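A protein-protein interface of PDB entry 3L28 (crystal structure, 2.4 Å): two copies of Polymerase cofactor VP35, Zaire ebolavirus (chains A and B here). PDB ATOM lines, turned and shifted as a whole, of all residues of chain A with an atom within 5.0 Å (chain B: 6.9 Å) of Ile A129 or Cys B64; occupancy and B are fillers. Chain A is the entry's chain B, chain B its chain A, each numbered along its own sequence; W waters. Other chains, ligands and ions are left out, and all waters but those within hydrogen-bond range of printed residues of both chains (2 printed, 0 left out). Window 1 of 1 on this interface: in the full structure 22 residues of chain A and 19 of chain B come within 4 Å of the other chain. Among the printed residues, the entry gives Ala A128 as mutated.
Printed residues of chain A that touch a printed residue of chain B: Phe A28, Asp A110, Arg A111, Gly A112, Trp A113, Ala A128 and Ile A129.
Hydrophobic or aromatic side chains of chain A within 4 Å of the printed part of chain B: Phe A28, Trp A113, Ala A128 and Ile A129.
Among the printed residues, Asp or Glu carboxylates within 4 Å of a Lys or Arg side-chain nitrogen of the other chain: Arg A111 with Asp B60.
Printed residues of chain B within 4 Å of Ala A128: Ser B61 (3.6 Å) and Gln B63 (3.4 Å).
Printed residues of chain B within 4 Å of Ile A129: Gln B63 and Cys B64.
Ser B55 touches none of the printed residues of chain A.
Of the printed residues of chain A, Asp B60 touches Arg A111 (2.9 Å).
Printed residues of chain A within 4 Å of Ser B61: Arg A111 (3.0 Å), Gly A112 (2.8 Å), Trp A113 (3.7 Å) and Ala A128 (3.6 Å).
Printed residues of chain A within 4 Å of Gln B63: Ala A128 and Ile A129.
Of the printed residues of chain A, Cys B64 touches Asp A110, Arg A111, Gly A112 and Ile A129.
Of the printed residues of chain A, Ile B129 touches Phe A28.
The nearest printed residue of chain A that does not touch Cys B64 is Trp A113 (6.0 Å).
The nearest printed residue of chain B that does not touch Arg A111 is Ser B55 (5.5 Å).
Phe A28 touches Ile B129, but with the chains exchanged Ile A129 does not touch Phe B28 (4.2 Å).
Of the 12 pairs that touch across the chains among the printed residues, none has its exchanged pair printed and touching as well.
Among the printed residues, merely in contact across the chains: Phe A28 with Ile B129 (3.9 Å), Asp A110 with Cys B64 (3.8 Å), Gly A112 with Cys B64 (3.7 Å), Trp A113 with Ser B61 (3.7 Å), Ala A128 with Ser B61 (3.6 Å), Ala A128 with Gln B63 (3.4 Å), Ile A129 with Gln B63 (3.3 Å) and Ile A129 with Cys B64 (3.9 Å).
O of Arg A111 lies close to SG of Cys B64.
The side-chain hydroxyl (OG) of Ser B61 is in hydrogen-bond range of the backbone carbonyl oxygen (O) of Gly A112, 2.8 Å away.
N of Ser B61 sits at hydrogen-bond distance from O of Arg A111.
OD1 of Asp B60 is in salt-bridge range of NE of Arg A111.
N of Asp B60 sits at hydrogen-bond distance from O of Ser B55 (3.0 Å).
N of Ile A129 lies within hydrogen-bond range of O of Gly A112, at 3.2 Å.
The backbone carbonyl oxygen (O) of Ala A128 sits at hydrogen-bond distance from the side-chain hydroxyl (OG) of Ser A99 (3.1 Å).
The side-chain carboxylate of Asp B60 sits at hydrogen-bond distance from the side-chain sulfur of Cys B64.
The side-chain hydroxyl (OG) of Ser B61 lies within hydrogen-bond range of the backbone NH (N) of Cys B64, 3.3 Å away.
Water W1 bridges the backbone carbonyl oxygen (O) of Asp A110 (2.7 Å) and the side-chain amide nitrogen (NE2) of Gln B68 (2.9 Å).
Water W2 lies within hydrogen-bond range of O of Asp A110 (3.0 Å) and SG of Cys B64 (3.3 Å).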
ATOM      1  N   ALA A  27     -15.740   2.119   2.170  1.00  0.00           N
ATOM      2  CA  ALA A  27     -15.711   1.660   3.559  1.00  0.00           C
ATOM      3  C   ALA A  27     -16.885   0.735   3.894  1.00  0.00           C
ATOM      4  O   ALA A  27     -16.732  -0.204   4.674  1.00  0.00           O
ATOM      5  CB  ALA A  27     -15.697   2.845   4.493  1.00  0.00           C
ATOM      6  N   PHE A  28     -18.048   1.010   3.299  1.00  0.00           N
ATOM      7  CA  PHE A  28     -19.239   0.167   3.450  1.00  0.00           C
ATOM      8  C   PHE A  28     -19.027  -1.243   2.893  1.00  0.00           C
ATOM      9  O   PHE A  28     -19.515  -2.214   3.463  1.00  0.00           O
ATOM     10  CB  PHE A  28     -20.455   0.821   2.784  1.00  0.00           C
ATOM     11  CG  PHE A  28     -20.835   2.146   3.381  1.00  0.00           C
ATOM     12  CD1 PHE A  28     -21.581   2.208   4.553  1.00  0.00           C
ATOM     13  CD2 PHE A  28     -20.447   3.331   2.773  1.00  0.00           C
ATOM     14  CE1 PHE A  28     -21.933   3.439   5.109  1.00  0.00           C
ATOM     15  CE2 PHE A  28     -20.794   4.564   3.318  1.00  0.00           C
ATOM     16  CZ  PHE A  28     -21.537   4.618   4.486  1.00  0.00           C
ATOM     17  N   LEU A  31     -16.973  -2.983   5.318  1.00  0.00           N
ATOM     18  CA  LEU A  31     -17.821  -3.203   6.490  1.00  0.00           C
ATOM     19  C   LEU A  31     -18.648  -4.491   6.394  1.00  0.00           C
ATOM     20  O   LEU A  31     -18.996  -5.086   7.415  1.00  0.00           O
ATOM     21  CB  LEU A  31     -18.722  -1.984   6.738  1.00  0.00           C
ATOM     22  CG  LEU A  31     -19.540  -1.886   8.034  1.00  0.00           C
ATOM     23  CD1 LEU A  31     -18.650  -1.871   9.280  1.00  0.00           C
ATOM     24  CD2 LEU A  31     -20.449  -0.660   8.011  1.00  0.00           C
ATOM     25  N   ILE A  67     -24.936   0.421   8.944  1.00  0.00           N
ATOM     26  CA  ILE A  67     -24.630   1.248  10.115  1.00  0.00           C
ATOM     27  C   ILE A  67     -25.559   0.907  11.280  1.00  0.00           C
ATOM     28  O   ILE A  67     -25.120   0.854  12.430  1.00  0.00           O
ATOM     29  CB  ILE A  67     -24.704   2.774   9.795  1.00  0.00           C
ATOM     30  CG1 ILE A  67     -23.719   3.161   8.683  1.00  0.00           C
ATOM     31  CG2 ILE A  67     -24.475   3.625  11.053  1.00  0.00           C
ATOM     32  CD1 ILE A  67     -22.304   2.615   8.849  1.00  0.00           C
ATOM     33  N   SER A  99     -10.449   8.058   2.834  1.00  0.00           N
ATOM     34  CA  SER A  99     -11.322   7.807   3.977  1.00  0.00           C
ATOM     35  C   SER A  99     -10.505   7.423   5.218  1.00  0.00           C
ATOM     36  O   SER A  99     -11.066   6.983   6.229  1.00  0.00           O
ATOM     37  CB  SER A  99     -12.326   6.702   3.619  1.00  0.00           C
ATOM     38  OG  SER A  99     -13.458   6.699   4.475  1.00  0.00           O
ATOM     39  N   ASP A 110     -19.053   1.074  16.180  1.00  0.00           N
ATOM     40  CA  ASP A 110     -20.272   1.892  16.233  1.00  0.00           C
ATOM     41  C   ASP A 110     -19.992   3.394  16.353  1.00  0.00           C
ATOM     42  O   ASP A 110     -20.908   4.217  16.271  1.00  0.00           O
ATOM     43  CB  ASP A 110     -21.215   1.414  17.349  1.00  0.00           C
ATOM     44  CG  ASP A 110     -20.569   1.420  18.739  1.00  0.00           C
ATOM     45  OD1 ASP A 110     -19.547   2.108  18.960  1.00  0.00           O
ATOM     46  OD2 ASP A 110     -21.108   0.732  19.631  1.00  0.00           O
ATOM     47  N   ARG A 111     -18.724   3.744  16.544  1.00  0.00           N
ATOM     48  CA  ARG A 111     -18.311   5.140  16.544  1.00  0.00           C
ATOM     49  C   ARG A 111     -17.852   5.566  15.148  1.00  0.00           C
ATOM     50  O   ARG A 111     -17.345   6.672  14.958  1.00  0.00           O
ATOM     51  CB  ARG A 111     -17.237   5.390  17.607  1.00  0.00           C
ATOM     52  CG  ARG A 111     -17.695   5.018  19.008  1.00  0.00           C
ATOM     53  CD  ARG A 111     -16.885   5.703  20.105  1.00  0.00           C
ATOM     54  NE  ARG A 111     -17.643   6.775  20.752  1.00  0.00           N
ATOM     55  CZ  ARG A 111     -18.549   6.588  21.711  1.00  0.00           C
ATOM     56  NH1 ARG A 111     -18.829   5.367  22.144  1.00  0.00           N
ATOM     57  NH2 ARG A 111     -19.184   7.627  22.232  1.00  0.00           N
ATOM     58  N   GLY A 112     -18.051   4.674  14.177  1.00  0.00           N
ATOM     59  CA  GLY A 112     -17.810   4.969  12.769  1.00  0.00           C
ATOM     60  C   GLY A 112     -16.452   4.528  12.263  1.00  0.00           C
ATOM     61  O   GLY A 112     -15.829   5.227  11.460  1.00  0.00           O
ATOM     62  N   TRP A 113     -16.001   3.366  12.729  1.00  0.00           N
ATOM     63  CA  TRP A 113     -14.697   2.834  12.350  1.00  0.00           C
ATOM     64  C   TRP A 113     -14.808   1.411  11.815  1.00  0.00           C
ATOM     65  O   TRP A 113     -15.172   0.486  12.542  1.00  0.00           O
ATOM     66  CB  TRP A 113     -13.712   2.916  13.524  1.00  0.00           C
ATOM     67  CG  TRP A 113     -13.445   4.325  13.961  1.00  0.00           C
ATOM     68  CD1 TRP A 113     -13.897   4.931  15.100  1.00  0.00           C
ATOM     69  CD2 TRP A 113     -12.691   5.319  13.250  1.00  0.00           C
ATOM     70  NE1 TRP A 113     -13.462   6.234  15.148  1.00  0.00           N
ATOM     71  CE2 TRP A 113     -12.721   6.499  14.026  1.00  0.00           C
ATOM     72  CE3 TRP A 113     -11.986   5.324  12.036  1.00  0.00           C
ATOM     73  CZ2 TRP A 113     -12.073   7.672  13.630  1.00  0.00           C
ATOM     74  CZ3 TRP A 113     -11.346   6.494  11.642  1.00  0.00           C
ATOM     75  CH2 TRP A 113     -11.391   7.649  12.439  1.00  0.00           C
ATOM     76  N   VAL A 114     -14.495   1.253  10.533  1.00  0.00           N
ATOM     77  CA  VAL A 114     -14.629  -0.028   9.848  1.00  0.00           C
ATOM     78  C   VAL A 114     -13.480  -0.967  10.214  1.00  0.00           C
ATOM     79  O   VAL A 114     -13.706  -2.088  10.676  1.00  0.00           O
ATOM     80  CB  VAL A 114     -14.720   0.155   8.316  1.00  0.00           C
ATOM     81  CG1 VAL A 114     -14.876  -1.185   7.628  1.00  0.00           C
ATOM     82  CG2 VAL A 114     -15.887   1.067   7.956  1.00  0.00           C
ATOM     83  N   LEU A 127      -9.868   3.374   9.038  1.00  0.00           N
ATOM     84  CA  LEU A 127     -10.864   3.494   7.979  1.00  0.00           C
ATOM     85  C   LEU A 127     -12.225   3.880   8.559  1.00  0.00           C
ATOM     86  O   LEU A 127     -12.896   3.066   9.200  1.00  0.00           O
ATOM     87  CB  LEU A 127     -10.968   2.200   7.162  1.00  0.00           C
ATOM     88  CG  LEU A 127     -11.959   2.216   5.996  1.00  0.00           C
ATOM     89  CD1 LEU A 127     -11.495   3.171   4.896  1.00  0.00           C
ATOM     90  CD2 LEU A 127     -12.190   0.811   5.446  1.00  0.00           C
ATOM     91  N   ALA A 128     -12.612   5.133   8.334  1.00  0.00           N
ATOM     92  CA  ALA A 128     -13.916   5.640   8.753  1.00  0.00           C
ATOM     93  C   ALA A 128     -14.995   5.149   7.793  1.00  0.00           C
ATOM     94  O   ALA A 128     -14.716   4.898   6.621  1.00  0.00           O
ATOM     95  CB  ALA A 128     -13.899   7.161   8.798  1.00  0.00           C
ATOM     96  N   ILE A 129     -16.222   5.016   8.294  1.00  0.00           N
ATOM     97  CA  ILE A 129     -17.368   4.625   7.467  1.00  0.00           C
ATOM     98  C   ILE A 129     -17.558   5.578   6.287  1.00  0.00           C
ATOM     99  O   ILE A 129     -17.123   6.730   6.334  1.00  0.00           O
ATOM    100  CB  ILE A 129     -18.687   4.551   8.278  1.00  0.00           C
ATOM    101  CG1 ILE A 129     -18.920   5.850   9.063  1.00  0.00           C
ATOM    102  CG2 ILE A 129     -18.676   3.339   9.200  1.00  0.00           C
ATOM    103  CD1 ILE A 129     -20.364   6.110   9.427  1.00  0.00           C
ATOM    104  OXT ILE A 129     -18.142   5.213   5.263  1.00  0.00           O
ATOM    105  N   LEU B  21     -13.294  16.194   6.316  1.00  0.00           N
ATOM    106  CA  LEU B  21     -13.690  15.289   5.240  1.00  0.00           C
ATOM    107  C   LEU B  21     -12.898  15.532   3.957  1.00  0.00           C
ATOM    108  O   LEU B  21     -13.277  16.378   3.146  1.00  0.00           O
ATOM    109  CB  LEU B  21     -15.199  15.399   4.967  1.00  0.00           C
ATOM    110  CG  LEU B  21     -16.177  15.051   6.094  1.00  0.00           C
ATOM    111  CD1 LEU B  21     -17.517  15.700   5.827  1.00  0.00           C
ATOM    112  CD2 LEU B  21     -16.331  13.548   6.266  1.00  0.00           C
ATOM    113  N   PHE B  28     -20.731  12.694   1.530  1.00  0.00           N
ATOM    114  CA  PHE B  28     -20.640  13.300   2.860  1.00  0.00           C
ATOM    115  C   PHE B  28     -20.452  14.816   2.854  1.00  0.00           C
ATOM    116  O   PHE B  28     -20.843  15.489   3.808  1.00  0.00           O
ATOM    117  CB  PHE B  28     -19.586  12.604   3.726  1.00  0.00           C
ATOM    118  CG  PHE B  28     -20.120  11.413   4.471  1.00  0.00           C
ATOM    119  CD1 PHE B  28     -20.985  11.584   5.545  1.00  0.00           C
ATOM    120  CD2 PHE B  28     -19.769  10.125   4.095  1.00  0.00           C
ATOM    121  CE1 PHE B  28     -21.489  10.491   6.235  1.00  0.00           C
ATOM    122  CE2 PHE B  28     -20.269   9.022   4.780  1.00  0.00           C
ATOM    123  CZ  PHE B  28     -21.131   9.207   5.851  1.00  0.00           C
ATOM    124  N   SER B  55     -19.006  14.656  19.502  1.00  0.00           N
ATOM    125  CA  SER B  55     -18.872  13.321  18.923  1.00  0.00           C
ATOM    126  C   SER B  55     -17.421  13.004  18.561  1.00  0.00           C
ATOM    127  O   SER B  55     -16.947  11.896  18.820  1.00  0.00           O
ATOM    128  CB  SER B  55     -19.792  13.157  17.712  1.00  0.00           C
ATOM    129  OG  SER B  55     -21.156  13.151  18.105  1.00  0.00           O
ATOM    130  N   ASP B  60     -15.488   9.512  17.760  1.00  0.00           N
ATOM    131  CA  ASP B  60     -16.270   9.240  16.551  1.00  0.00           C
ATOM    132  C   ASP B  60     -15.543   9.759  15.326  1.00  0.00           C
ATOM    133  O   ASP B  60     -14.867  10.792  15.385  1.00  0.00           O
ATOM    134  CB  ASP B  60     -17.649   9.910  16.603  1.00  0.00           C
ATOM    135  CG  ASP B  60     -18.598   9.262  17.598  1.00  0.00           C
ATOM    136  OD1 ASP B  60     -18.203   8.324  18.324  1.00  0.00           O
ATOM    137  OD2 ASP B  60     -19.759   9.713  17.658  1.00  0.00           O
ATOM    138  N   SER B  61     -15.691   9.048  14.211  1.00  0.00           N
ATOM    139  CA  SER B  61     -15.275   9.582  12.920  1.00  0.00           C
ATOM    140  C   SER B  61     -16.224  10.723  12.547  1.00  0.00           C
ATOM    141  O   SER B  61     -17.378  10.729  12.984  1.00  0.00           O
ATOM    142  CB  SER B  61     -15.278   8.492  11.849  1.00  0.00           C
ATOM    143  OG  SER B  61     -16.555   7.894  11.710  1.00  0.00           O
ATOM    144  N   PRO B  62     -15.741  11.708  11.764  1.00  0.00           N
ATOM    145  CA  PRO B  62     -16.604  12.811  11.315  1.00  0.00           C
ATOM    146  C   PRO B  62     -17.848  12.320  10.570  1.00  0.00           C
ATOM    147  O   PRO B  62     -18.913  12.930  10.681  1.00  0.00           O
ATOM    148  CB  PRO B  62     -15.696  13.601  10.368  1.00  0.00           C
ATOM    149  CG  PRO B  62     -14.319  13.281  10.821  1.00  0.00           C
ATOM    150  CD  PRO B  62     -14.360  11.861  11.271  1.00  0.00           C
ATOM    151  N   GLN B  63     -17.702  11.224   9.827  1.00  0.00           N
ATOM    152  CA  GLN B  63     -18.811  10.601   9.104  1.00  0.00           C
ATOM    153  C   GLN B  63     -19.889  10.106  10.068  1.00  0.00           C
ATOM    154  O   GLN B  63     -21.076  10.329   9.850  1.00  0.00           O
ATOM    155  CB  GLN B  63     -18.303   9.453   8.223  1.00  0.00           C
ATOM    156  CG  GLN B  63     -17.451   9.892   7.034  1.00  0.00           C
ATOM    157  CD  GLN B  63     -15.970  10.027   7.357  1.00  0.00           C
ATOM    158  OE1 GLN B  63     -15.576  10.147   8.515  1.00  0.00           O
ATOM    159  NE2 GLN B  63     -15.141  10.012   6.321  1.00  0.00           N
ATOM    160  N   CYS B  64     -19.462   9.449  11.142  1.00  0.00           N
ATOM    161  CA  CYS B  64     -20.367   9.001  12.195  1.00  0.00           C
ATOM    162  C   CYS B  64     -21.049  10.169  12.916  1.00  0.00           C
ATOM    163  O   CYS B  64     -22.243  10.108  13.214  1.00  0.00           O
ATOM    164  CB  CYS B  64     -19.611   8.144  13.206  1.00  0.00           C
ATOM    165  SG  CYS B  64     -20.589   7.664  14.626  1.00  0.00           S
ATOM    166  N   ALA B  65     -20.276  11.219  13.191  1.00  0.00           N
ATOM    167  CA  ALA B  65     -20.775  12.429  13.842  1.00  0.00           C
ATOM    168  C   ALA B  65     -21.930  13.059  13.068  1.00  0.00           C
ATOM    169  O   ALA B  65     -22.946  13.434  13.658  1.00  0.00           O
ATOM    170  CB  ALA B  65     -19.643  13.435  14.022  1.00  0.00           C
ATOM    171  N   LEU B  66     -21.770  13.161  11.749  1.00  0.00           N
ATOM    172  CA  LEU B  66     -22.804  13.716  10.873  1.00  0.00           C
ATOM    173  C   LEU B  66     -24.069  12.862  10.830  1.00  0.00           C
ATOM    174  O   LEU B  66     -25.174  13.404  10.834  1.00  0.00           O
ATOM    175  CB  LEU B  66     -22.261  13.934   9.458  1.00  0.00           C
ATOM    176  CG  LEU B  66     -21.151  14.974   9.278  1.00  0.00           C
ATOM    177  CD1 LEU B  66     -20.531  14.853   7.900  1.00  0.00           C
ATOM    178  CD2 LEU B  66     -21.662  16.385   9.514  1.00  0.00           C
ATOM    179  N   ILE B  67     -23.904  11.537  10.795  1.00  0.00           N
ATOM    180  CA  ILE B  67     -25.045  10.609  10.805  1.00  0.00           C
ATOM    181  C   ILE B  67     -25.815  10.706  12.127  1.00  0.00           C
ATOM    182  O   ILE B  67     -27.046  10.598  12.157  1.00  0.00           O
ATOM    183  CB  ILE B  67     -24.615   9.131  10.538  1.00  0.00           C
ATOM    184  CG1 ILE B  67     -23.864   8.986   9.201  1.00  0.00           C
ATOM    185  CG2 ILE B  67     -25.820   8.178  10.593  1.00  0.00           C
ATOM    186  CD1 ILE B  67     -24.588   9.528   7.971  1.00  0.00           C
ATOM    187  N   GLN B  68     -25.075  10.922  13.211  1.00  0.00           N
ATOM    188  CA  GLN B  68     -25.662  11.066  14.537  1.00  0.00           C
ATOM    189  C   GLN B  68     -26.479  12.356  14.642  1.00  0.00           C
ATOM    190  O   GLN B  68     -27.503  12.388  15.320  1.00  0.00           O
ATOM    191  CB  GLN B  68     -24.568  11.013  15.609  1.00  0.00           C
ATOM    192  CG  GLN B  68     -24.976  10.302  16.895  1.00  0.00           C
ATOM    193  CD  GLN B  68     -25.061   8.789  16.748  1.00  0.00           C
ATOM    194  OE1 GLN B  68     -25.934   8.263  16.052  1.00  0.00           O
ATOM    195  NE2 GLN B  68     -24.162   8.081  17.422  1.00  0.00           N
ATOM    196  N   ILE B  69     -26.023  13.405  13.957  1.00  0.00           N
ATOM    197  CA  ILE B  69     -26.751  14.678  13.865  1.00  0.00           C
ATOM    198  C   ILE B  69     -28.105  14.514  13.157  1.00  0.00           C
ATOM    199  O   ILE B  69     -29.124  15.019  13.644  1.00  0.00           O
ATOM    200  CB  ILE B  69     -25.892  15.780  13.178  1.00  0.00           C
ATOM    201  CG1 ILE B  69     -24.825  16.308  14.145  1.00  0.00           C
ATOM    202  CG2 ILE B  69     -26.758  16.940  12.681  1.00  0.00           C
ATOM    203  CD1 ILE B  69     -23.584  16.871  13.463  1.00  0.00           C
ATOM    204  N   ILE B 129     -25.953   7.855   1.484  1.00  0.00           N
ATOM    205  CA  ILE B 129     -24.751   8.247   2.225  1.00  0.00           C
ATOM    206  C   ILE B 129     -23.520   7.465   1.755  1.00  0.00           C
ATOM    207  O   ILE B 129     -23.640   6.390   1.164  1.00  0.00           O
ATOM    208  CB  ILE B 129     -24.927   8.071   3.753  1.00  0.00           C
ATOM    209  CG1 ILE B 129     -25.436   6.659   4.085  1.00  0.00           C
ATOM    210  CG2 ILE B 129     -25.857   9.151   4.313  1.00  0.00           C
ATOM    211  CD1 ILE B 129     -25.100   6.185   5.490  1.00  0.00           C
ATOM    212  OXT ILE B 129     -22.379   7.887   1.943  1.00  0.00           O
HETATM  213  O   HOH W   1     -22.527   5.707  17.835  1.00  0.00           O
HETATM  214  O   HOH W   2     -21.460   4.688  13.369  1.00  0.00           O
